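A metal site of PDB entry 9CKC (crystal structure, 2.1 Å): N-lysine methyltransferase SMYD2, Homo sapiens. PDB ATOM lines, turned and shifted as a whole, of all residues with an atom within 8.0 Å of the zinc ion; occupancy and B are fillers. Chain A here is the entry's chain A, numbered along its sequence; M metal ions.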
ATOM      1  N   HIS A  51      29.977 -13.606  18.780  1.00  0.00           N
ATOM      2  CA  HIS A  51      30.533 -13.637  17.438  1.00  0.00           C
ATOM      3  C   HIS A  51      29.544 -13.075  16.441  1.00  0.00           C
ATOM      4  O   HIS A  51      28.322 -13.213  16.598  1.00  0.00           O
ATOM      5  CB  HIS A  51      30.903 -15.076  17.027  1.00  0.00           C
ATOM      6  CG  HIS A  51      32.011 -15.683  17.831  1.00  0.00           C
ATOM      7  ND1 HIS A  51      33.297 -15.799  17.364  1.00  0.00           N
ATOM      8  CD2 HIS A  51      32.021 -16.198  19.088  1.00  0.00           C
ATOM      9  CE1 HIS A  51      34.059 -16.368  18.284  1.00  0.00           C
ATOM     10  NE2 HIS A  51      33.309 -16.623  19.339  1.00  0.00           N
ATOM     11  N   CYS A  52      30.071 -12.452  15.387  1.00  0.00           N
ATOM     12  CA  CYS A  52      29.232 -11.991  14.288  1.00  0.00           C
ATOM     13  C   CYS A  52      28.752 -13.178  13.468  1.00  0.00           C
ATOM     14  O   CYS A  52      29.546 -14.037  13.077  1.00  0.00           O
ATOM     15  CB  CYS A  52      30.019 -11.024  13.409  1.00  0.00           C
ATOM     16  SG  CYS A  52      29.207 -10.559  11.863  1.00  0.00           S
ATOM     17  N   GLU A  53      27.439 -13.200  13.173  1.00  0.00           N
ATOM     18  CA  GLU A  53      26.872 -14.332  12.438  1.00  0.00           C
ATOM     19  C   GLU A  53      27.505 -14.477  11.061  1.00  0.00           C
ATOM     20  O   GLU A  53      27.704 -15.596  10.578  1.00  0.00           O
ATOM     21  CB  GLU A  53      25.359 -14.162  12.307  1.00  0.00           C
ATOM     22  CG  GLU A  53      24.591 -14.139  13.622  1.00  0.00           C
ATOM     23  CD  GLU A  53      24.120 -15.523  14.064  1.00  0.00           C
ATOM     24  OE1 GLU A  53      24.026 -16.430  13.212  1.00  0.00           O
ATOM     25  OE2 GLU A  53      23.838 -15.679  15.266  1.00  0.00           O
ATOM     26  N   TYR A  54      27.843 -13.357  10.416  1.00  0.00           N
ATOM     27  CA  TYR A  54      28.318 -13.414   9.039  1.00  0.00           C
ATOM     28  C   TYR A  54      29.781 -13.843   8.946  1.00  0.00           C
ATOM     29  O   TYR A  54      30.116 -14.789   8.236  1.00  0.00           O
ATOM     30  CB  TYR A  54      28.130 -12.054   8.346  1.00  0.00           C
ATOM     31  CG  TYR A  54      28.574 -12.098   6.906  1.00  0.00           C
ATOM     32  CD1 TYR A  54      27.917 -12.918   5.994  1.00  0.00           C
ATOM     33  CD2 TYR A  54      29.647 -11.341   6.467  1.00  0.00           C
ATOM     34  CE1 TYR A  54      28.311 -12.971   4.675  1.00  0.00           C
ATOM     35  CE2 TYR A  54      30.055 -11.392   5.144  1.00  0.00           C
ATOM     36  CZ  TYR A  54      29.381 -12.205   4.255  1.00  0.00           C
ATOM     37  OH  TYR A  54      29.776 -12.258   2.936  1.00  0.00           O
ATOM     38  N   CYS A  55      30.672 -13.140   9.655  1.00  0.00           N
ATOM     39  CA  CYS A  55      32.106 -13.316   9.471  1.00  0.00           C
ATOM     40  C   CYS A  55      32.806 -13.983  10.658  1.00  0.00           C
ATOM     41  O   CYS A  55      34.016 -14.211  10.590  1.00  0.00           O
ATOM     42  CB  CYS A  55      32.763 -11.964   9.191  1.00  0.00           C
ATOM     43  SG  CYS A  55      32.861 -10.917  10.638  1.00  0.00           S
ATOM     44  N   PHE A  56      32.069 -14.287  11.726  1.00  0.00           N
ATOM     45  CA  PHE A  56      32.527 -15.048  12.905  1.00  0.00           C
ATOM     46  C   PHE A  56      33.499 -14.277  13.784  1.00  0.00           C
ATOM     47  O   PHE A  56      34.064 -14.864  14.714  1.00  0.00           O
ATOM     48  CB  PHE A  56      33.147 -16.388  12.506  1.00  0.00           C
ATOM     49  CG  PHE A  56      32.145 -17.492  12.282  1.00  0.00           C
ATOM     50  CD1 PHE A  56      30.875 -17.206  11.801  1.00  0.00           C
ATOM     51  CD2 PHE A  56      32.471 -18.809  12.566  1.00  0.00           C
ATOM     52  CE1 PHE A  56      29.953 -18.224  11.590  1.00  0.00           C
ATOM     53  CE2 PHE A  56      31.557 -19.823  12.359  1.00  0.00           C
ATOM     54  CZ  PHE A  56      30.297 -19.526  11.868  1.00  0.00           C
ATOM     55  N   THR A  57      33.702 -12.991  13.530  1.00  0.00           N
ATOM     56  CA  THR A  57      34.602 -12.184  14.349  1.00  0.00           C
ATOM     57  C   THR A  57      34.066 -12.041  15.768  1.00  0.00           C
ATOM     58  O   THR A  57      32.918 -11.650  15.974  1.00  0.00           O
ATOM     59  CB  THR A  57      34.786 -10.795  13.722  1.00  0.00           C
ATOM     60  OG1 THR A  57      35.275 -10.945  12.386  1.00  0.00           O
ATOM     61  CG2 THR A  57      35.766  -9.972  14.540  1.00  0.00           C
ATOM     62  N   ARG A  58      34.912 -12.341  16.743  1.00  0.00           N
ATOM     63  CA  ARG A  58      34.588 -12.169  18.159  1.00  0.00           C
ATOM     64  C   ARG A  58      34.925 -10.746  18.578  1.00  0.00           C
ATOM     65  O   ARG A  58      36.060 -10.292  18.394  1.00  0.00           O
ATOM     66  CB  ARG A  58      35.359 -13.178  19.006  1.00  0.00           C
ATOM     67  CG  ARG A  58      34.978 -13.177  20.477  1.00  0.00           C
ATOM     68  CD  ARG A  58      35.879 -14.101  21.284  1.00  0.00           C
ATOM     69  NE  ARG A  58      37.295 -13.879  21.004  1.00  0.00           N
ATOM     70  CZ  ARG A  58      38.111 -14.788  20.470  1.00  0.00           C
ATOM     71  NH1 ARG A  58      37.665 -15.997  20.156  1.00  0.00           N
ATOM     72  NH2 ARG A  58      39.390 -14.480  20.258  1.00  0.00           N
ATOM     73  N   LYS A  59      33.938 -10.037  19.125  1.00  0.00           N
ATOM     74  CA  LYS A  59      34.161  -8.698  19.658  1.00  0.00           C
ATOM     75  C   LYS A  59      32.987  -8.323  20.541  1.00  0.00           C
ATOM     76  O   LYS A  59      31.928  -8.959  20.511  1.00  0.00           O
ATOM     77  CB  LYS A  59      34.335  -7.666  18.529  1.00  0.00           C
ATOM     78  CG  LYS A  59      33.142  -7.575  17.601  1.00  0.00           C
ATOM     79  CD  LYS A  59      33.238  -6.384  16.667  1.00  0.00           C
ATOM     80  CE  LYS A  59      34.356  -6.567  15.669  1.00  0.00           C
ATOM     81  NZ  LYS A  59      34.393  -5.458  14.673  1.00  0.00           N
ATOM     82  N   LEU A  62      28.348  -6.015  19.544  1.00  0.00           N
ATOM     83  CA  LEU A  62      27.837  -6.378  18.240  1.00  0.00           C
ATOM     84  C   LEU A  62      26.412  -5.851  18.062  1.00  0.00           C
ATOM     85  O   LEU A  62      25.624  -5.830  19.012  1.00  0.00           O
ATOM     86  CB  LEU A  62      27.858  -7.897  18.059  1.00  0.00           C
ATOM     87  CG  LEU A  62      29.242  -8.560  17.965  1.00  0.00           C
ATOM     88  CD1 LEU A  62      29.154 -10.058  18.179  1.00  0.00           C
ATOM     89  CD2 LEU A  62      29.863  -8.262  16.607  1.00  0.00           C
ATOM     90  N   PHE A  72      23.697 -11.461  16.033  1.00  0.00           N
ATOM     91  CA  PHE A  72      24.507 -10.273  16.251  1.00  0.00           C
ATOM     92  C   PHE A  72      25.504 -10.107  15.116  1.00  0.00           C
ATOM     93  O   PHE A  72      25.929 -11.085  14.502  1.00  0.00           O
ATOM     94  CB  PHE A  72      25.220 -10.348  17.612  1.00  0.00           C
ATOM     95  CG  PHE A  72      24.285 -10.360  18.786  1.00  0.00           C
ATOM     96  CD1 PHE A  72      23.571 -11.505  19.123  1.00  0.00           C
ATOM     97  CD2 PHE A  72      24.103  -9.222  19.562  1.00  0.00           C
ATOM     98  CE1 PHE A  72      22.711 -11.522  20.199  1.00  0.00           C
ATOM     99  CE2 PHE A  72      23.237  -9.236  20.646  1.00  0.00           C
ATOM    100  CZ  PHE A  72      22.547 -10.385  20.963  1.00  0.00           C
ATOM    101  N   TYR A  73      25.860  -8.858  14.829  1.00  0.00           N
ATOM    102  CA  TYR A  73      26.655  -8.523  13.652  1.00  0.00           C
ATOM    103  C   TYR A  73      27.657  -7.427  13.967  1.00  0.00           C
ATOM    104  O   TYR A  73      27.456  -6.619  14.877  1.00  0.00           O
ATOM    105  CB  TYR A  73      25.751  -8.059  12.495  1.00  0.00           C
ATOM    106  CG  TYR A  73      24.806  -9.129  12.022  1.00  0.00           C
ATOM    107  CD1 TYR A  73      25.255 -10.176  11.234  1.00  0.00           C
ATOM    108  CD2 TYR A  73      23.456  -9.099  12.362  1.00  0.00           C
ATOM    109  CE1 TYR A  73      24.403 -11.157  10.795  1.00  0.00           C
ATOM    110  CE2 TYR A  73      22.585 -10.079  11.935  1.00  0.00           C
ATOM    111  CZ  TYR A  73      23.060 -11.105  11.145  1.00  0.00           C
ATOM    112  OH  TYR A  73      22.211 -12.094  10.710  1.00  0.00           O
ATOM    113  N   CYS A  74      28.743  -7.406  13.193  1.00  0.00           N
ATOM    114  CA  CYS A  74      29.718  -6.318  13.303  1.00  0.00           C
ATOM    115  C   CYS A  74      29.073  -4.970  12.980  1.00  0.00           C
ATOM    116  O   CYS A  74      29.316  -3.987  13.683  1.00  0.00           O
ATOM    117  CB  CYS A  74      30.898  -6.580  12.361  1.00  0.00           C
ATOM    118  SG  CYS A  74      31.830  -8.100  12.686  1.00  0.00           S
ATOM    119  N   ASN A  75      28.250  -4.918  11.941  1.00  0.00           N
ATOM    120  CA  ASN A  75      27.691  -3.672  11.409  1.00  0.00           C
ATOM    121  C   ASN A  75      26.561  -4.037  10.450  1.00  0.00           C
ATOM    122  O   ASN A  75      26.235  -5.223  10.286  1.00  0.00           O
ATOM    123  CB  ASN A  75      28.782  -2.852  10.735  1.00  0.00           C
ATOM    124  CG  ASN A  75      29.603  -3.665   9.758  1.00  0.00           C
ATOM    125  OD1 ASN A  75      29.063  -4.216   8.798  1.00  0.00           O
ATOM    126  ND2 ASN A  75      30.906  -3.779  10.016  1.00  0.00           N
ATOM    127  N   GLU A  77      26.580  -3.837   7.237  1.00  0.00           N
ATOM    128  CA  GLU A  77      27.087  -4.553   6.064  1.00  0.00           C
ATOM    129  C   GLU A  77      27.104  -6.062   6.316  1.00  0.00           C
ATOM    130  O   GLU A  77      26.587  -6.842   5.511  1.00  0.00           O
ATOM    131  CB  GLU A  77      28.480  -4.059   5.680  1.00  0.00           C
ATOM    132  CG  GLU A  77      28.920  -4.519   4.301  1.00  0.00           C
ATOM    133  CD  GLU A  77      30.348  -4.146   3.980  1.00  0.00           C
ATOM    134  OE1 GLU A  77      30.821  -3.118   4.510  1.00  0.00           O
ATOM    135  OE2 GLU A  77      31.007  -4.896   3.236  1.00  0.00           O
ATOM    136  N   CYS A  78      27.722  -6.487   7.429  1.00  0.00           N
ATOM    137  CA  CYS A  78      27.661  -7.898   7.795  1.00  0.00           C
ATOM    138  C   CYS A  78      26.222  -8.365   7.940  1.00  0.00           C
ATOM    139  O   CYS A  78      25.872  -9.469   7.494  1.00  0.00           O
ATOM    140  CB  CYS A  78      28.441  -8.132   9.092  1.00  0.00           C
ATOM    141  SG  CYS A  78      30.240  -8.322   8.884  1.00  0.00           S
ATOM    142  N   GLN A  79      25.364  -7.533   8.534  1.00  0.00           N
ATOM    143  CA  GLN A  79      23.960  -7.884   8.689  1.00  0.00           C
ATOM    144  C   GLN A  79      23.274  -8.075   7.334  1.00  0.00           C
ATOM    145  O   GLN A  79      22.521  -9.032   7.142  1.00  0.00           O
ATOM    146  CB  GLN A  79      23.238  -6.810   9.508  1.00  0.00           C
ATOM    147  CG  GLN A  79      21.767  -7.070   9.737  1.00  0.00           C
ATOM    148  CD  GLN A  79      21.172  -6.076  10.694  1.00  0.00           C
ATOM    149  OE1 GLN A  79      21.833  -5.132  11.129  1.00  0.00           O
ATOM    150  NE2 GLN A  79      19.891  -6.261  11.015  1.00  0.00           N
HETATM  151 ZN    ZN M   1      31.090  -9.379  10.829  1.00  0.00          ZN
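Of the 17 residues printed, 4 come within 4 Å of the zinc ion.
The side-chain sulfur (SG) of Cys 55 binds the zinc ion.
The side-chain sulfur (SG) of Cys 78 binds the zinc ion, 2.4 Å away.
The zinc ion is bound by the side-chain sulfur (SG) of Cys 74 (2.4 Å).
SG of Cys 52 is bound to the zinc ion.
SG of Cys 52 sits close to N of Tyr 54 (3.4 Å).
N of Cys 52 sits at hydrogen-bond distance from O of Thr 57 (3.0 Å).
The backbone NH (N) of Cys 78 is in hydrogen-bond range of the side-chain amide oxygen (OD1) of Asn 75, 3.0 Å away.
SG of Cys 55 sits close to OG1 of Thr 57.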
